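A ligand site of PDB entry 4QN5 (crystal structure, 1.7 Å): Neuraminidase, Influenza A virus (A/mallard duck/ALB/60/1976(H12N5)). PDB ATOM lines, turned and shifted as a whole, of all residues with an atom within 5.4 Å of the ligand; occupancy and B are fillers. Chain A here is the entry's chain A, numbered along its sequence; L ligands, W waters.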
ATOM      1  N   ARG A  37      24.144  18.693  22.402  1.00  0.00           N
ATOM      2  CA  ARG A  37      23.772  18.359  23.769  1.00  0.00           C
ATOM      3  C   ARG A  37      22.796  17.195  23.710  1.00  0.00           C
ATOM      4  O   ARG A  37      22.441  16.739  22.623  1.00  0.00           O
ATOM      5  CB  ARG A  37      23.146  19.554  24.512  1.00  0.00           C
ATOM      6  CG  ARG A  37      24.133  20.285  25.423  1.00  0.00           C
ATOM      7  CD  ARG A  37      23.436  20.846  26.658  1.00  0.00           C
ATOM      8  NE  ARG A  37      22.924  19.779  27.508  1.00  0.00           N
ATOM      9  CZ  ARG A  37      21.936  19.924  28.382  1.00  0.00           C
ATOM     10  NH1 ARG A  37      21.326  21.086  28.509  1.00  0.00           N
ATOM     11  NH2 ARG A  37      21.546  18.881  29.114  1.00  0.00           N
ATOM     12  N   GLU A  38      22.392  16.695  24.873  1.00  0.00           N
ATOM     13  CA  GLU A  38      21.437  15.600  24.919  1.00  0.00           C
ATOM     14  C   GLU A  38      21.924  14.389  24.132  1.00  0.00           C
ATOM     15  O   GLU A  38      21.191  13.851  23.296  1.00  0.00           O
ATOM     16  CB  GLU A  38      20.072  16.056  24.412  1.00  0.00           C
ATOM     17  CG  GLU A  38      19.385  17.119  25.279  1.00  0.00           C
ATOM     18  CD  GLU A  38      19.787  18.544  24.931  1.00  0.00           C
ATOM     19  OE1 GLU A  38      19.814  19.390  25.847  1.00  0.00           O
ATOM     20  OE2 GLU A  38      20.055  18.821  23.739  1.00  0.00           O
ATOM     21  N   ASP A  70      17.924  26.104  23.850  1.00  0.00           N
ATOM     22  CA  ASP A  70      17.482  24.713  23.752  1.00  0.00           C
ATOM     23  C   ASP A  70      16.798  24.331  22.448  1.00  0.00           C
ATOM     24  O   ASP A  70      16.896  23.182  21.998  1.00  0.00           O
ATOM     25  CB  ASP A  70      16.566  24.367  24.932  1.00  0.00           C
ATOM     26  CG  ASP A  70      17.312  24.237  26.241  1.00  0.00           C
ATOM     27  OD1 ASP A  70      18.529  23.964  26.208  1.00  0.00           O
ATOM     28  OD2 ASP A  70      16.679  24.412  27.312  1.00  0.00           O
ATOM     29  N   ARG A  71      16.075  25.275  21.845  1.00  0.00           N
ATOM     30  CA  ARG A  71      15.294  24.971  20.649  1.00  0.00           C
ATOM     31  C   ARG A  71      15.549  25.960  19.510  1.00  0.00           C
ATOM     32  O   ARG A  71      15.547  27.174  19.714  1.00  0.00           O
ATOM     33  CB  ARG A  71      13.804  24.912  20.988  1.00  0.00           C
ATOM     34  CG  ARG A  71      13.492  23.918  22.112  1.00  0.00           C
ATOM     35  CD  ARG A  71      12.014  23.911  22.492  1.00  0.00           C
ATOM     36  NE  ARG A  71      11.568  25.212  22.982  1.00  0.00           N
ATOM     37  CZ  ARG A  71      11.844  25.688  24.199  1.00  0.00           C
ATOM     38  NH1 ARG A  71      12.590  24.986  25.040  1.00  0.00           N
ATOM     39  NH2 ARG A  71      11.403  26.880  24.558  1.00  0.00           N
ATOM     40  N   ARG A  75      18.568  22.587  14.885  1.00  0.00           N
ATOM     41  CA  ARG A  75      18.922  21.390  15.628  1.00  0.00           C
ATOM     42  C   ARG A  75      18.453  20.135  14.900  1.00  0.00           C
ATOM     43  O   ARG A  75      17.347  20.101  14.347  1.00  0.00           O
ATOM     44  CB  ARG A  75      18.335  21.425  17.044  1.00  0.00           C
ATOM     45  CG  ARG A  75      18.772  22.635  17.843  1.00  0.00           C
ATOM     46  CD  ARG A  75      18.711  22.352  19.347  1.00  0.00           C
ATOM     47  NE  ARG A  75      19.791  21.470  19.786  1.00  0.00           N
ATOM     48  CZ  ARG A  75      20.008  21.121  21.056  1.00  0.00           C
ATOM     49  NH1 ARG A  75      19.207  21.579  22.000  1.00  0.00           N
ATOM     50  NH2 ARG A  75      21.016  20.320  21.371  1.00  0.00           N
ATOM     51  N   TRP A  98      14.636  19.148  17.987  1.00  0.00           N
ATOM     52  CA  TRP A  98      15.197  19.739  19.205  1.00  0.00           C
ATOM     53  C   TRP A  98      14.816  18.931  20.448  1.00  0.00           C
ATOM     54  O   TRP A  98      15.125  19.310  21.579  1.00  0.00           O
ATOM     55  CB  TRP A  98      14.869  21.227  19.351  1.00  0.00           C
ATOM     56  CG  TRP A  98      13.461  21.685  19.035  1.00  0.00           C
ATOM     57  CD1 TRP A  98      13.073  22.450  17.968  1.00  0.00           C
ATOM     58  CD2 TRP A  98      12.271  21.441  19.803  1.00  0.00           C
ATOM     59  NE1 TRP A  98      11.716  22.682  18.023  1.00  0.00           N
ATOM     60  CE2 TRP A  98      11.207  22.073  19.138  1.00  0.00           C
ATOM     61  CE3 TRP A  98      12.005  20.739  20.982  1.00  0.00           C
ATOM     62  CZ2 TRP A  98       9.893  22.039  19.608  1.00  0.00           C
ATOM     63  CZ3 TRP A  98      10.700  20.699  21.462  1.00  0.00           C
ATOM     64  CH2 TRP A  98       9.664  21.346  20.771  1.00  0.00           C
ATOM     65  N   SER A  99      14.154  17.803  20.226  1.00  0.00           N
ATOM     66  CA  SER A  99      13.912  16.796  21.261  1.00  0.00           C
ATOM     67  C   SER A  99      13.719  15.469  20.542  1.00  0.00           C
ATOM     68  O   SER A  99      13.113  15.449  19.472  1.00  0.00           O
ATOM     69  CB  SER A  99      12.667  17.149  22.080  1.00  0.00           C
ATOM     70  OG  SER A  99      12.444  16.181  23.103  1.00  0.00           O
ATOM     71  N   ILE A 142       5.318  23.107  23.996  1.00  0.00           N
ATOM     72  CA  ILE A 142       6.596  22.417  23.895  1.00  0.00           C
ATOM     73  C   ILE A 142       6.473  20.903  24.055  1.00  0.00           C
ATOM     74  O   ILE A 142       6.924  20.326  25.048  1.00  0.00           O
ATOM     75  CB  ILE A 142       7.624  22.971  24.910  1.00  0.00           C
ATOM     76  CG1 ILE A 142       7.633  24.500  24.876  1.00  0.00           C
ATOM     77  CG2 ILE A 142       9.024  22.427  24.599  1.00  0.00           C
ATOM     78  CD1 ILE A 142       8.644  25.113  25.808  1.00  0.00           C
ATOM     79  N   LEU A 143       5.858  20.264  23.068  1.00  0.00           N
ATOM     80  CA  LEU A 143       5.870  18.808  22.984  1.00  0.00           C
ATOM     81  C   LEU A 143       7.320  18.346  23.120  1.00  0.00           C
ATOM     82  O   LEU A 143       8.204  18.907  22.474  1.00  0.00           O
ATOM     83  CB  LEU A 143       5.293  18.374  21.639  1.00  0.00           C
ATOM     84  CG  LEU A 143       5.300  16.881  21.314  1.00  0.00           C
ATOM     85  CD1 LEU A 143       4.420  16.113  22.290  1.00  0.00           C
ATOM     86  CD2 LEU A 143       4.837  16.647  19.891  1.00  0.00           C
ATOM     87  N   ARG A 144       7.570  17.356  23.962  1.00  0.00           N
ATOM     88  CA  ARG A 144       8.940  16.935  24.241  1.00  0.00           C
ATOM     89  C   ARG A 144       9.024  15.463  24.650  1.00  0.00           C
ATOM     90  O   ARG A 144       8.046  14.892  25.123  1.00  0.00           O
ATOM     91  CB  ARG A 144       9.588  17.837  25.288  1.00  0.00           C
ATOM     92  CG  ARG A 144       8.792  18.015  26.591  1.00  0.00           C
ATOM     93  CD  ARG A 144       9.195  19.295  27.287  1.00  0.00           C
ATOM     94  NE  ARG A 144       8.621  19.453  28.624  1.00  0.00           N
ATOM     95  CZ  ARG A 144       7.437  20.014  28.864  1.00  0.00           C
ATOM     96  NH1 ARG A 144       6.684  20.463  27.865  1.00  0.00           N
ATOM     97  NH2 ARG A 144       6.993  20.121  30.110  1.00  0.00           N
ATOM     98  N   GLU A 147      14.924  12.113  25.199  1.00  0.00           N
ATOM     99  CA  GLU A 147      16.357  12.381  25.055  1.00  0.00           C
ATOM    100  C   GLU A 147      17.175  11.166  25.465  1.00  0.00           C
ATOM    101  O   GLU A 147      18.299  11.286  25.942  1.00  0.00           O
ATOM    102  CB  GLU A 147      16.802  13.607  25.867  1.00  0.00           C
ATOM    103  CG  GLU A 147      15.776  14.727  25.984  1.00  0.00           C
ATOM    104  CD  GLU A 147      15.420  15.346  24.639  1.00  0.00           C
ATOM    105  OE1 GLU A 147      15.914  14.869  23.606  1.00  0.00           O
ATOM    106  OE2 GLU A 147      14.636  16.322  24.648  1.00  0.00           O
ATOM    107  N   ALA A 166       6.448  23.664  32.182  1.00  0.00           N
ATOM    108  CA  ALA A 166       7.692  23.112  32.713  1.00  0.00           C
ATOM    109  C   ALA A 166       7.668  23.055  34.239  1.00  0.00           C
ATOM    110  O   ALA A 166       8.330  22.217  34.846  1.00  0.00           O
ATOM    111  CB  ALA A 166       8.874  23.938  32.230  1.00  0.00           C
ATOM    112  N   GLU A 196       9.227  14.173  32.872  1.00  0.00           N
ATOM    113  CA  GLU A 196       9.962  14.603  31.693  1.00  0.00           C
ATOM    114  C   GLU A 196      11.157  13.685  31.472  1.00  0.00           C
ATOM    115  O   GLU A 196      11.641  13.060  32.409  1.00  0.00           O
ATOM    116  CB  GLU A 196      10.474  16.028  31.843  1.00  0.00           C
ATOM    117  CG  GLU A 196       9.413  17.095  31.866  1.00  0.00           C
ATOM    118  CD  GLU A 196       9.999  18.488  31.955  1.00  0.00           C
ATOM    119  OE1 GLU A 196       9.328  19.448  31.532  1.00  0.00           O
ATOM    120  OE2 GLU A 196      11.155  18.607  32.425  1.00  0.00           O
ATOM    121  N   GLU A 197      11.630  13.643  30.229  1.00  0.00           N
ATOM    122  CA  GLU A 197      12.912  13.008  29.913  1.00  0.00           C
ATOM    123  C   GLU A 197      13.099  11.641  30.552  1.00  0.00           C
ATOM    124  O   GLU A 197      14.109  11.393  31.220  1.00  0.00           O
ATOM    125  CB  GLU A 197      14.054  13.957  30.305  1.00  0.00           C
ATOM    126  CG  GLU A 197      14.024  15.259  29.524  1.00  0.00           C
ATOM    127  CD  GLU A 197      15.005  16.290  30.040  1.00  0.00           C
ATOM    128  OE1 GLU A 197      15.417  16.198  31.207  1.00  0.00           O
ATOM    129  OE2 GLU A 197      15.349  17.206  29.261  1.00  0.00           O
ATOM    130  N   ARG A 212      12.290  12.591  35.199  1.00  0.00           N
ATOM    131  CA  ARG A 212      12.632  13.858  35.828  1.00  0.00           C
ATOM    132  C   ARG A 212      11.347  14.607  36.194  1.00  0.00           C
ATOM    133  O   ARG A 212      10.471  14.787  35.351  1.00  0.00           O
ATOM    134  CB  ARG A 212      13.480  14.701  34.883  1.00  0.00           C
ATOM    135  CG  ARG A 212      13.581  16.187  35.215  1.00  0.00           C
ATOM    136  CD  ARG A 212      14.372  16.907  34.132  1.00  0.00           C
ATOM    137  NE  ARG A 212      14.446  18.359  34.314  1.00  0.00           N
ATOM    138  CZ  ARG A 212      15.189  19.163  33.568  1.00  0.00           C
ATOM    139  NH1 ARG A 212      15.935  18.659  32.591  1.00  0.00           N
ATOM    140  NH2 ARG A 212      15.196  20.470  33.790  1.00  0.00           N
ATOM    141  N   ASN A 214      10.121  18.158  37.122  1.00  0.00           N
ATOM    142  CA  ASN A 214      10.637  19.520  37.038  1.00  0.00           C
ATOM    143  C   ASN A 214       9.757  20.497  37.823  1.00  0.00           C
ATOM    144  O   ASN A 214       9.819  21.711  37.625  1.00  0.00           O
ATOM    145  CB  ASN A 214      10.731  19.968  35.576  1.00  0.00           C
ATOM    146  CG  ASN A 214      11.835  20.981  35.334  1.00  0.00           C
ATOM    147  OD1 ASN A 214      13.009  20.710  35.593  1.00  0.00           O
ATOM    148  ND2 ASN A 214      11.466  22.144  34.828  1.00  0.00           N
ATOM    149  N   TYR A 268      13.079  22.761  39.069  1.00  0.00           N
ATOM    150  CA  TYR A 268      14.181  22.361  38.200  1.00  0.00           C
ATOM    151  C   TYR A 268      14.447  20.881  38.356  1.00  0.00           C
ATOM    152  O   TYR A 268      13.736  20.194  39.064  1.00  0.00           O
ATOM    153  CB  TYR A 268      15.443  23.189  38.477  1.00  0.00           C
ATOM    154  CG  TYR A 268      16.350  23.322  37.269  1.00  0.00           C
ATOM    155  CD1 TYR A 268      15.849  23.747  36.042  1.00  0.00           C
ATOM    156  CD2 TYR A 268      17.705  23.038  37.357  1.00  0.00           C
ATOM    157  CE1 TYR A 268      16.670  23.885  34.939  1.00  0.00           C
ATOM    158  CE2 TYR A 268      18.536  23.173  36.245  1.00  0.00           C
ATOM    159  CZ  TYR A 268      18.011  23.593  35.045  1.00  0.00           C
ATOM    160  OH  TYR A 268      18.832  23.731  33.943  1.00  0.00           O
ATOM    161  N   GLY A 269      15.477  20.395  37.680  1.00  0.00           N
ATOM    162  CA  GLY A 269      15.822  18.991  37.734  1.00  0.00           C
ATOM    163  C   GLY A 269      16.844  18.680  36.670  1.00  0.00           C
ATOM    164  O   GLY A 269      17.310  19.578  35.980  1.00  0.00           O
ATOM    165  N   ARG A 292      25.042  20.629  38.330  1.00  0.00           N
ATOM    166  CA  ARG A 292      25.371  19.458  37.538  1.00  0.00           C
ATOM    167  C   ARG A 292      26.887  19.260  37.562  1.00  0.00           C
ATOM    168  O   ARG A 292      27.584  19.559  36.601  1.00  0.00           O
ATOM    169  CB  ARG A 292      24.831  19.605  36.125  1.00  0.00           C
ATOM    170  CG  ARG A 292      23.317  19.665  36.117  1.00  0.00           C
ATOM    171  CD  ARG A 292      22.749  20.255  34.842  1.00  0.00           C
ATOM    172  NE  ARG A 292      21.288  20.236  34.875  1.00  0.00           N
ATOM    173  CZ  ARG A 292      20.507  20.505  33.832  1.00  0.00           C
ATOM    174  NH1 ARG A 292      21.041  20.833  32.669  1.00  0.00           N
ATOM    175  NH2 ARG A 292      19.181  20.446  33.970  1.00  0.00           N
ATOM    176  N   TYR A 326      23.123  15.503  31.922  1.00  0.00           N
ATOM    177  CA  TYR A 326      22.139  14.442  31.768  1.00  0.00           C
ATOM    178  C   TYR A 326      22.792  13.060  31.891  1.00  0.00           C
ATOM    179  O   TYR A 326      23.982  12.898  31.661  1.00  0.00           O
ATOM    180  CB  TYR A 326      21.461  14.529  30.405  1.00  0.00           C
ATOM    181  CG  TYR A 326      20.384  15.585  30.302  1.00  0.00           C
ATOM    182  CD1 TYR A 326      20.217  16.536  31.303  1.00  0.00           C
ATOM    183  CD2 TYR A 326      19.527  15.618  29.211  1.00  0.00           C
ATOM    184  CE1 TYR A 326      19.227  17.494  31.210  1.00  0.00           C
ATOM    185  CE2 TYR A 326      18.538  16.578  29.109  1.00  0.00           C
ATOM    186  CZ  TYR A 326      18.385  17.510  30.117  1.00  0.00           C
ATOM    187  OH  TYR A 326      17.408  18.472  30.026  1.00  0.00           O
HETATM  188  C1  LIG L   1      17.917  21.372  30.682  1.00  0.00           C
HETATM  189  C2  LIG L   1      16.927  21.521  29.550  1.00  0.00           C
HETATM  190  C3  LIG L   1      17.574  21.090  28.231  1.00  0.00           C
HETATM  191  C4  LIG L   1      16.560  20.494  27.271  1.00  0.00           C
HETATM  192  C5  LIG L   1      15.171  21.062  27.505  1.00  0.00           C
HETATM  193  C6  LIG L   1      14.716  20.690  28.911  1.00  0.00           C
HETATM  194  C7  LIG L   1      13.527  21.525  29.402  1.00  0.00           C
HETATM  195  C8  LIG L   1      13.130  21.063  30.796  1.00  0.00           C
HETATM  196  C9  LIG L   1      11.848  21.744  31.263  1.00  0.00           C
HETATM  197  C10 LIG L   1      13.519  21.210  25.699  1.00  0.00           C
HETATM  198  C11 LIG L   1      12.618  20.429  24.786  1.00  0.00           C
HETATM  199  N1  LIG L   1      14.242  20.483  26.545  1.00  0.00           N
HETATM  200  O1  LIG L   1      17.479  21.182  31.836  1.00  0.00           O
HETATM  201  O2  LIG L   1      19.140  21.447  30.426  1.00  0.00           O
HETATM  202  O3  LIG L   1      16.550  22.903  29.459  1.00  0.00           O
HETATM  203  O4  LIG L   1      16.953  20.804  25.921  1.00  0.00           O
HETATM  204  O5  LIG L   1      15.784  20.734  29.870  1.00  0.00           O
HETATM  205  O6  LIG L   1      13.868  22.912  29.420  1.00  0.00           O
HETATM  206  O7  LIG L   1      12.930  19.647  30.764  1.00  0.00           O
HETATM  207  O8  LIG L   1      10.755  21.309  30.457  1.00  0.00           O
HETATM  208  O9  LIG L   1      13.572  22.427  25.664  1.00  0.00           O
HETATM  209  O   HOH W   1      11.828  18.026  28.709  1.00  0.00           O
HETATM  210  O   HOH W   2      16.061  18.824  24.093  1.00  0.00           O
HETATM  211  O   HOH W   3      17.690  24.609  31.400  1.00  0.00           O
HETATM  212  O   HOH W   4      11.820  23.946  27.892  1.00  0.00           O
HETATM  213  O   HOH W   5      20.055  21.998  24.882  1.00  0.00           O
HETATM  214  O   HOH W   6      13.941  17.626  26.972  1.00  0.00           O
HETATM  215  O   HOH W   7       9.497  22.841  28.673  1.00  0.00           O
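OE1 of Glu 196 lies within hydrogen-bond range of O8 of the ligand (2.6 Å).
An oxygen (O5) of the ligand lies within hydrogen-bond range of the side-chain hydroxyl (OH) of Tyr 326 (2.8 Å).
An oxygen (O9) of the ligand sits at hydrogen-bond distance from the guanidinium group (NH1) of Arg 71, 2.8 Å away.
The guanidinium group (NE) of Arg 144 lies within hydrogen-bond range of an oxygen (O8) of the ligand.
An oxygen (O3) of the ligand lies within hydrogen-bond range of the side-chain carboxylate of Asp 70, 2.6 Å away.
NH2 of Arg 292 lies within salt-bridge range of O1 of the ligand, 2.8 Å away.
The guanidinium group (NH1) of Arg 212 is in salt-bridge range of an oxygen (O1) of the ligand.
An oxygen (O2) of the ligand lies within salt-bridge range of the guanidinium group of Arg 37, at 2.9 Å.
The side-chain carboxylate (OE1) of Glu 38 lies within hydrogen-bond range of an oxygen (O4) of the ligand (3.2 Å).
Water W7 bridges O8 of the ligand and NE of Arg 144.
Water W4 bridges O6 of the ligand (2.8 Å) and NH1 of Arg 71 (3.1 Å).
Water W3 bridges an oxygen (O3) of the ligand and the side-chain hydroxyl (OH) of Tyr 268.
Water W2 lies within hydrogen-bond range of the backbone carbonyl oxygen (O) of Trp 98 (2.7 Å), an oxygen (O4) of the ligand (2.8 Å) and the side-chain carboxylate (OE2) of Glu 147 (2.9 Å).
Water W6 lies within hydrogen-bond range of the side-chain carboxylate (OE2) of Glu 197 (2.7 Å), the side-chain carboxylate (OE2) of Glu 147 (2.8 Å) and a nitrogen (N1) of the ligand (2.9 Å).
Water W5 lies within hydrogen-bond range of OE1 of Glu 38 (2.8 Å), OD1 of Asp 70 (2.8 Å), NH1 of Arg 75 (3.0 Å) and O4 of the ligand (3.5 Å).
Trp 98 touches the ligand (CZ3 to C11, 3.8 Å).
CB of Ala 166 touches O8 of the ligand (3.7 Å).
OE2 of Glu 197 touches C6 of the ligand, at 3.6 Å.
ND2 of Asn 214 touches C9 of the ligand, 3.6 Å away.
Tyr 268 touches the ligand (OH to O1, 3.6 Å).
Hydrophobic or aromatic side chains that line the ligand: Trp 98, Ala 166 and Tyr 326.
Of the 20 residues printed, 14 come within 4 Å of the ligand.
The side-chain hydroxyl (OH) of Tyr 326 lies within hydrogen-bond range of the guanidinium group (NH1) of Arg 212 (3.0 Å).
The side-chain amide oxygen of Asn 214 is in hydrogen-bond range of the guanidinium group of Arg 212.
OD1 of Asn 214 is in hydrogen-bond range of N of Gly 269, 3.2 Å away.
The guanidinium group of Arg 144 lies within hydrogen-bond range of the backbone carbonyl oxygen of Ile 142 (2.8 Å).
The guanidinium group (NH2) of Arg 75 lies within salt-bridge range of the side-chain carboxylate (OE2) of Glu 38 (3.0 Å).
The side-chain carboxylate (OE1) of Glu 38 lies within salt-bridge range of the guanidinium group (NH1) of Arg 37, at 3.5 Å.
O of Ala 166 sits at hydrogen-bond distance from ND2 of Asn 214 (3.1 Å).
NH2 of Arg 212 sits at hydrogen-bond distance from O of Gly 269 (3.2 Å).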
